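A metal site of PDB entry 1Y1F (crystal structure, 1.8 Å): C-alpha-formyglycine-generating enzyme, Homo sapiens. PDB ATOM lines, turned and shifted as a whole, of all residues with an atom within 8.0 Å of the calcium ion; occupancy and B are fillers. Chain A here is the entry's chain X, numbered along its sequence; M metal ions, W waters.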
ATOM      1  N   TYR A  57      -2.378 -24.178  20.015  1.00  0.00           N
ATOM      2  CA  TYR A  57      -1.511 -25.248  20.519  1.00  0.00           C
ATOM      3  C   TYR A  57      -0.711 -25.874  19.395  1.00  0.00           C
ATOM      4  O   TYR A  57      -1.176 -25.953  18.233  1.00  0.00           O
ATOM      5  CB  TYR A  57      -2.368 -26.377  21.154  1.00  0.00           C
ATOM      6  CG  TYR A  57      -3.396 -25.918  22.185  1.00  0.00           C
ATOM      7  CD1 TYR A  57      -2.986 -25.430  23.422  1.00  0.00           C
ATOM      8  CD2 TYR A  57      -4.767 -25.990  21.919  1.00  0.00           C
ATOM      9  CE1 TYR A  57      -3.891 -24.997  24.354  1.00  0.00           C
ATOM     10  CE2 TYR A  57      -5.706 -25.549  22.858  1.00  0.00           C
ATOM     11  CZ  TYR A  57      -5.253 -25.065  24.083  1.00  0.00           C
ATOM     12  OH  TYR A  57      -6.172 -24.632  25.032  1.00  0.00           O
ATOM     13  N   GLU A  58       0.468 -26.384  19.742  1.00  0.00           N
ATOM     14  CA  GLU A  58       1.155 -27.344  18.880  1.00  0.00           C
ATOM     15  C   GLU A  58       0.202 -28.496  18.581  1.00  0.00           C
ATOM     16  O   GLU A  58      -0.592 -28.914  19.429  1.00  0.00           O
ATOM     17  CB  GLU A  58       2.412 -27.895  19.582  1.00  0.00           C
ATOM     18  CG  GLU A  58       3.494 -26.824  19.885  1.00  0.00           C
ATOM     19  CD  GLU A  58       4.387 -27.144  21.068  1.00  0.00           C
ATOM     20  OE1 GLU A  58       3.888 -27.794  22.008  1.00  0.00           O
ATOM     21  OE2 GLU A  58       5.599 -26.768  21.060  1.00  0.00           O
ATOM     22  N   PRO A 133       2.873 -32.653  22.131  1.00  0.00           N
ATOM     23  CA  PRO A 133       3.027 -32.379  20.718  1.00  0.00           C
ATOM     24  C   PRO A 133       3.513 -33.587  19.932  1.00  0.00           C
ATOM     25  O   PRO A 133       4.338 -34.361  20.414  1.00  0.00           O
ATOM     26  CB  PRO A 133       4.102 -31.285  20.698  1.00  0.00           C
ATOM     27  CG  PRO A 133       4.872 -31.491  21.955  1.00  0.00           C
ATOM     28  CD  PRO A 133       3.819 -31.852  22.941  1.00  0.00           C
ATOM     29  N   TRP A 159       4.275 -16.429  11.929  1.00  0.00           N
ATOM     30  CA  TRP A 159       4.719 -17.125  13.129  1.00  0.00           C
ATOM     31  C   TRP A 159       5.362 -16.184  14.141  1.00  0.00           C
ATOM     32  O   TRP A 159       4.958 -16.151  15.334  1.00  0.00           O
ATOM     33  CB  TRP A 159       5.637 -18.319  12.788  1.00  0.00           C
ATOM     34  CG  TRP A 159       5.903 -19.229  13.953  1.00  0.00           C
ATOM     35  CD1 TRP A 159       5.307 -20.417  14.212  1.00  0.00           C
ATOM     36  CD2 TRP A 159       6.794 -18.980  15.068  1.00  0.00           C
ATOM     37  NE1 TRP A 159       5.788 -20.954  15.393  1.00  0.00           N
ATOM     38  CE2 TRP A 159       6.687 -20.072  15.934  1.00  0.00           C
ATOM     39  CE3 TRP A 159       7.680 -17.946  15.385  1.00  0.00           C
ATOM     40  CZ2 TRP A 159       7.418 -20.160  17.114  1.00  0.00           C
ATOM     41  CZ3 TRP A 159       8.402 -18.030  16.553  1.00  0.00           C
ATOM     42  CH2 TRP A 159       8.246 -19.115  17.419  1.00  0.00           C
ATOM     43  N   ASN A 187       8.791 -24.516  28.299  1.00  0.00           N
ATOM     44  CA  ASN A 187       9.490 -25.748  28.496  1.00  0.00           C
ATOM     45  C   ASN A 187      10.804 -25.753  27.688  1.00  0.00           C
ATOM     46  O   ASN A 187      10.819 -26.017  26.481  1.00  0.00           O
ATOM     47  CB  ASN A 187       8.598 -26.928  28.156  1.00  0.00           C
ATOM     48  CG  ASN A 187       9.321 -28.261  28.306  1.00  0.00           C
ATOM     49  OD1 ASN A 187      10.255 -28.373  29.096  1.00  0.00           O
ATOM     50  ND2 ASN A 187       8.874 -29.292  27.565  1.00  0.00           N
ATOM     51  N   TYR A 220       0.033 -21.050  23.244  1.00  0.00           N
ATOM     52  CA  TYR A 220       0.725 -21.889  24.226  1.00  0.00           C
ATOM     53  C   TYR A 220       1.982 -22.469  23.593  1.00  0.00           C
ATOM     54  O   TYR A 220       1.931 -22.954  22.485  1.00  0.00           O
ATOM     55  CB  TYR A 220      -0.183 -23.038  24.687  1.00  0.00           C
ATOM     56  CG  TYR A 220      -1.362 -22.566  25.497  1.00  0.00           C
ATOM     57  CD1 TYR A 220      -2.468 -22.004  24.882  1.00  0.00           C
ATOM     58  CD2 TYR A 220      -1.309 -22.579  26.898  1.00  0.00           C
ATOM     59  CE1 TYR A 220      -3.526 -21.502  25.647  1.00  0.00           C
ATOM     60  CE2 TYR A 220      -2.360 -22.098  27.661  1.00  0.00           C
ATOM     61  CZ  TYR A 220      -3.462 -21.562  27.035  1.00  0.00           C
ATOM     62  OH  TYR A 220      -4.484 -21.113  27.830  1.00  0.00           O
ATOM     63  N   ASN A 221       3.099 -22.419  24.303  1.00  0.00           N
ATOM     64  CA  ASN A 221       4.336 -23.126  23.917  1.00  0.00           C
ATOM     65  C   ASN A 221       4.877 -22.752  22.556  1.00  0.00           C
ATOM     66  O   ASN A 221       5.485 -23.552  21.859  1.00  0.00           O
ATOM     67  CB  ASN A 221       4.169 -24.651  24.066  1.00  0.00           C
ATOM     68  CG  ASN A 221       3.799 -25.014  25.482  1.00  0.00           C
ATOM     69  OD1 ASN A 221       4.598 -24.788  26.414  1.00  0.00           O
ATOM     70  ND2 ASN A 221       2.580 -25.539  25.659  1.00  0.00           N
ATOM     71  N   ILE A 222       4.694 -21.485  22.227  1.00  0.00           N
ATOM     72  CA  ILE A 222       5.169 -20.934  20.957  1.00  0.00           C
ATOM     73  C   ILE A 222       6.711 -20.845  21.000  1.00  0.00           C
ATOM     74  O   ILE A 222       7.363 -21.084  20.007  1.00  0.00           O
ATOM     75  CB  ILE A 222       4.430 -19.616  20.593  1.00  0.00           C
ATOM     76  CG1 ILE A 222       4.785 -19.208  19.157  1.00  0.00           C
ATOM     77  CG2 ILE A 222       4.746 -18.464  21.573  1.00  0.00           C
ATOM     78  CD1 ILE A 222       3.763 -19.455  18.156  1.00  0.00           C
ATOM     79  N   VAL A 223       7.296 -20.508  22.144  1.00  0.00           N
ATOM     80  CA  VAL A 223       8.710 -20.831  22.391  1.00  0.00           C
ATOM     81  C   VAL A 223       8.811 -22.068  23.292  1.00  0.00           C
ATOM     82  O   VAL A 223       7.949 -22.319  24.177  1.00  0.00           O
ATOM     83  CB  VAL A 223       9.594 -19.644  22.896  1.00  0.00           C
ATOM     84  CG1 VAL A 223       9.499 -18.465  21.989  1.00  0.00           C
ATOM     85  CG2 VAL A 223       9.247 -19.249  24.356  1.00  0.00           C
ATOM     86  N   GLY A 224       9.828 -22.870  23.032  1.00  0.00           N
ATOM     87  CA  GLY A 224      10.020 -24.127  23.735  1.00  0.00           C
ATOM     88  C   GLY A 224       9.076 -25.243  23.389  1.00  0.00           C
ATOM     89  O   GLY A 224       8.265 -25.130  22.473  1.00  0.00           O
ATOM     90  N   ASN A 225       9.202 -26.334  24.152  1.00  0.00           N
ATOM     91  CA  ASN A 225       8.467 -27.589  23.957  1.00  0.00           C
ATOM     92  C   ASN A 225       8.918 -28.237  22.665  1.00  0.00           C
ATOM     93  O   ASN A 225      10.026 -28.750  22.618  1.00  0.00           O
ATOM     94  CB  ASN A 225       6.948 -27.379  24.097  1.00  0.00           C
ATOM     95  CG  ASN A 225       6.247 -28.582  24.746  1.00  0.00           C
ATOM     96  OD1 ASN A 225       6.833 -29.321  25.539  1.00  0.00           O
ATOM     97  ND2 ASN A 225       4.958 -28.745  24.432  1.00  0.00           N
ATOM     98  N   ALA A 226       8.139 -28.173  21.598  1.00  0.00           N
ATOM     99  CA  ALA A 226       8.619 -28.583  20.282  1.00  0.00           C
ATOM    100  C   ALA A 226       8.999 -27.387  19.397  1.00  0.00           C
ATOM    101  O   ALA A 226       8.314 -26.362  19.408  1.00  0.00           O
ATOM    102  CB  ALA A 226       7.555 -29.431  19.597  1.00  0.00           C
ATOM    103  N   TRP A 227      10.064 -27.512  18.621  1.00  0.00           N
ATOM    104  CA  TRP A 227      10.286 -26.643  17.460  1.00  0.00           C
ATOM    105  C   TRP A 227       9.073 -26.658  16.535  1.00  0.00           C
ATOM    106  O   TRP A 227       8.293 -27.623  16.503  1.00  0.00           O
ATOM    107  CB  TRP A 227      11.458 -27.143  16.619  1.00  0.00           C
ATOM    108  CG  TRP A 227      12.795 -26.720  17.069  1.00  0.00           C
ATOM    109  CD1 TRP A 227      13.692 -27.489  17.751  1.00  0.00           C
ATOM    110  CD2 TRP A 227      13.475 -25.483  16.778  1.00  0.00           C
ATOM    111  NE1 TRP A 227      14.870 -26.794  17.969  1.00  0.00           N
ATOM    112  CE2 TRP A 227      14.766 -25.557  17.368  1.00  0.00           C
ATOM    113  CE3 TRP A 227      13.135 -24.328  16.063  1.00  0.00           C
ATOM    114  CZ2 TRP A 227      15.685 -24.499  17.301  1.00  0.00           C
ATOM    115  CZ3 TRP A 227      14.048 -23.275  16.025  1.00  0.00           C
ATOM    116  CH2 TRP A 227      15.297 -23.376  16.608  1.00  0.00           C
ATOM    117  N   GLU A 228       8.921 -25.605  15.742  1.00  0.00           N
ATOM    118  CA  GLU A 228       7.767 -25.483  14.865  1.00  0.00           C
ATOM    119  C   GLU A 228       8.118 -25.142  13.420  1.00  0.00           C
ATOM    120  O   GLU A 228       8.762 -24.140  13.142  1.00  0.00           O
ATOM    121  CB  GLU A 228       6.773 -24.490  15.476  1.00  0.00           C
ATOM    122  CG  GLU A 228       6.468 -24.875  16.930  1.00  0.00           C
ATOM    123  CD  GLU A 228       5.467 -23.971  17.641  1.00  0.00           C
ATOM    124  OE1 GLU A 228       4.832 -23.115  17.013  1.00  0.00           O
ATOM    125  OE2 GLU A 228       5.330 -24.169  18.874  1.00  0.00           O
ATOM    126  N   LYS A 258      11.065 -22.493  13.834  1.00  0.00           N
ATOM    127  CA  LYS A 258      11.068 -21.450  14.848  1.00  0.00           C
ATOM    128  C   LYS A 258      10.750 -21.933  16.254  1.00  0.00           C
ATOM    129  O   LYS A 258      10.079 -22.965  16.462  1.00  0.00           O
ATOM    130  CB  LYS A 258      10.039 -20.372  14.490  1.00  0.00           C
ATOM    131  CG  LYS A 258      10.243 -19.619  13.173  1.00  0.00           C
ATOM    132  CD  LYS A 258      11.307 -18.529  13.195  1.00  0.00           C
ATOM    133  CE  LYS A 258      10.783 -17.200  13.710  1.00  0.00           C
ATOM    134  NZ  LYS A 258      11.842 -16.068  13.555  1.00  0.00           N
ATOM    135  N   GLY A 259      11.212 -21.155  17.240  1.00  0.00           N
ATOM    136  CA  GLY A 259      10.675 -21.239  18.591  1.00  0.00           C
ATOM    137  C   GLY A 259      11.477 -21.988  19.640  1.00  0.00           C
ATOM    138  O   GLY A 259      11.292 -21.750  20.847  1.00  0.00           O
ATOM    139  N   GLY A 260      12.379 -22.861  19.208  1.00  0.00           N
ATOM    140  CA  GLY A 260      13.154 -23.661  20.128  1.00  0.00           C
ATOM    141  C   GLY A 260      12.313 -24.746  20.758  1.00  0.00           C
ATOM    142  O   GLY A 260      11.116 -24.879  20.480  1.00  0.00           O
ATOM    143  N   SER A 261      12.963 -25.520  21.621  1.00  0.00           N
ATOM    144  CA  SER A 261      12.426 -26.767  22.121  1.00  0.00           C
ATOM    145  C   SER A 261      12.792 -26.992  23.571  1.00  0.00           C
ATOM    146  O   SER A 261      13.566 -26.231  24.151  1.00  0.00           O
ATOM    147  CB  SER A 261      12.926 -27.940  21.275  1.00  0.00           C
ATOM    148  OG  SER A 261      14.231 -28.389  21.652  1.00  0.00           O
ATOM    149  N   TYR A 262      12.255 -28.081  24.137  1.00  0.00           N
ATOM    150  CA  TYR A 262      12.655 -28.537  25.467  1.00  0.00           C
ATOM    151  C   TYR A 262      14.147 -28.784  25.668  1.00  0.00           C
ATOM    152  O   TYR A 262      14.592 -28.889  26.822  1.00  0.00           O
ATOM    153  CB  TYR A 262      11.886 -29.801  25.862  1.00  0.00           C
ATOM    154  CG  TYR A 262      12.206 -31.043  25.080  1.00  0.00           C
ATOM    155  CD1 TYR A 262      11.445 -31.412  23.964  1.00  0.00           C
ATOM    156  CD2 TYR A 262      13.245 -31.865  25.458  1.00  0.00           C
ATOM    157  CE1 TYR A 262      11.741 -32.598  23.242  1.00  0.00           C
ATOM    158  CE2 TYR A 262      13.561 -33.023  24.748  1.00  0.00           C
ATOM    159  CZ  TYR A 262      12.794 -33.389  23.645  1.00  0.00           C
ATOM    160  OH  TYR A 262      13.101 -34.563  22.972  1.00  0.00           O
ATOM    161  N   ASN A 288      12.458 -33.425  18.697  1.00  0.00           N
ATOM    162  CA  ASN A 288      12.119 -32.103  19.262  1.00  0.00           C
ATOM    163  C   ASN A 288      11.459 -31.146  18.287  1.00  0.00           C
ATOM    164  O   ASN A 288      11.437 -29.931  18.519  1.00  0.00           O
ATOM    165  CB  ASN A 288      13.380 -31.445  19.844  1.00  0.00           C
ATOM    166  CG  ASN A 288      14.365 -31.034  18.769  1.00  0.00           C
ATOM    167  OD1 ASN A 288      14.227 -31.416  17.619  1.00  0.00           O
ATOM    168  ND2 ASN A 288      15.378 -30.264  19.155  1.00  0.00           N
ATOM    169  N   GLY A 290       8.111 -30.271  15.867  1.00  0.00           N
ATOM    170  CA  GLY A 290       6.687 -30.384  15.607  1.00  0.00           C
ATOM    171  C   GLY A 290       6.206 -29.207  14.782  1.00  0.00           C
ATOM    172  O   GLY A 290       6.952 -28.640  13.950  1.00  0.00           O
ATOM    173  N   PHE A 291       4.956 -28.803  15.022  1.00  0.00           N
ATOM    174  CA  PHE A 291       4.313 -27.752  14.275  1.00  0.00           C
ATOM    175  C   PHE A 291       2.952 -27.386  14.788  1.00  0.00           C
ATOM    176  O   PHE A 291       2.347 -28.123  15.561  1.00  0.00           O
ATOM    177  CB  PHE A 291       4.167 -28.088  12.768  1.00  0.00           C
ATOM    178  CG  PHE A 291       3.184 -29.197  12.466  1.00  0.00           C
ATOM    179  CD1 PHE A 291       1.935 -28.901  11.952  1.00  0.00           C
ATOM    180  CD2 PHE A 291       3.494 -30.511  12.731  1.00  0.00           C
ATOM    181  CE1 PHE A 291       1.026 -29.902  11.661  1.00  0.00           C
ATOM    182  CE2 PHE A 291       2.565 -31.530  12.456  1.00  0.00           C
ATOM    183  CZ  PHE A 291       1.338 -31.211  11.934  1.00  0.00           C
ATOM    184  N   ARG A 292       2.489 -26.234  14.330  1.00  0.00           N
ATOM    185  CA  ARG A 292       1.100 -25.798  14.514  1.00  0.00           C
ATOM    186  C   ARG A 292       0.612 -25.214  13.177  1.00  0.00           C
ATOM    187  O   ARG A 292       1.417 -24.825  12.329  1.00  0.00           O
ATOM    188  CB  ARG A 292       0.972 -24.771  15.628  1.00  0.00           C
ATOM    189  CG  ARG A 292       1.363 -23.330  15.260  1.00  0.00           C
ATOM    190  CD  ARG A 292       1.165 -22.399  16.487  1.00  0.00           C
ATOM    191  NE  ARG A 292       2.097 -22.740  17.551  1.00  0.00           N
ATOM    192  CZ  ARG A 292       1.822 -22.745  18.865  1.00  0.00           C
ATOM    193  NH1 ARG A 292       0.617 -22.431  19.319  1.00  0.00           N
ATOM    194  NH2 ARG A 292       2.766 -23.086  19.710  1.00  0.00           N
HETATM  195 CA    CA M   1       6.788 -24.913  20.550  1.00  0.00          CA
HETATM  196  O   HOH W   1       8.573 -23.522  19.815  1.00  0.00           O
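The calcium ion is bound by the side-chain carboxylate of Glu 58 (2.3 Å), the backbone carbonyl oxygen of Asn 221 (2.3 Å), the side-chain carboxylate of Glu 228 (2.3 Å), water W1 (2.4 Å), the backbone carbonyl oxygen of Ala 226 (2.4 Å) and the backbone carbonyl oxygen of Gly 224 (2.4 Å).
Ile 222 touches the calcium ion.
Six residues have an atom within 4 Å of the calcium ion: Glu 58, Asn 221, Ile 222, Gly 224, Ala 226 and Glu 228.
The side-chain amide nitrogen (ND2) of Asn 225 lies within hydrogen-bond range of the side-chain carboxylate (OE1) of Glu 58, 2.8 Å away.
NH2 of Arg 292 lies close to O of Asn 221 (3.5 Å).
The guanidinium group (NE) of Arg 292 is in salt-bridge range of the side-chain carboxylate (OE1) of Glu 228 (2.8 Å).
O of Glu 228 is in hydrogen-bond range of N of Lys 258 (2.9 Å).
The indole nitrogen of Trp 159 lies within hydrogen-bond range of the side-chain carboxylate of Glu 228, 2.9 Å away.
O of Gly 260 lies within hydrogen-bond range of N of Gly 224 (3.5 Å).
O of Gly 259 lies within hydrogen-bond range of N of Gly 224 (2.9 Å).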
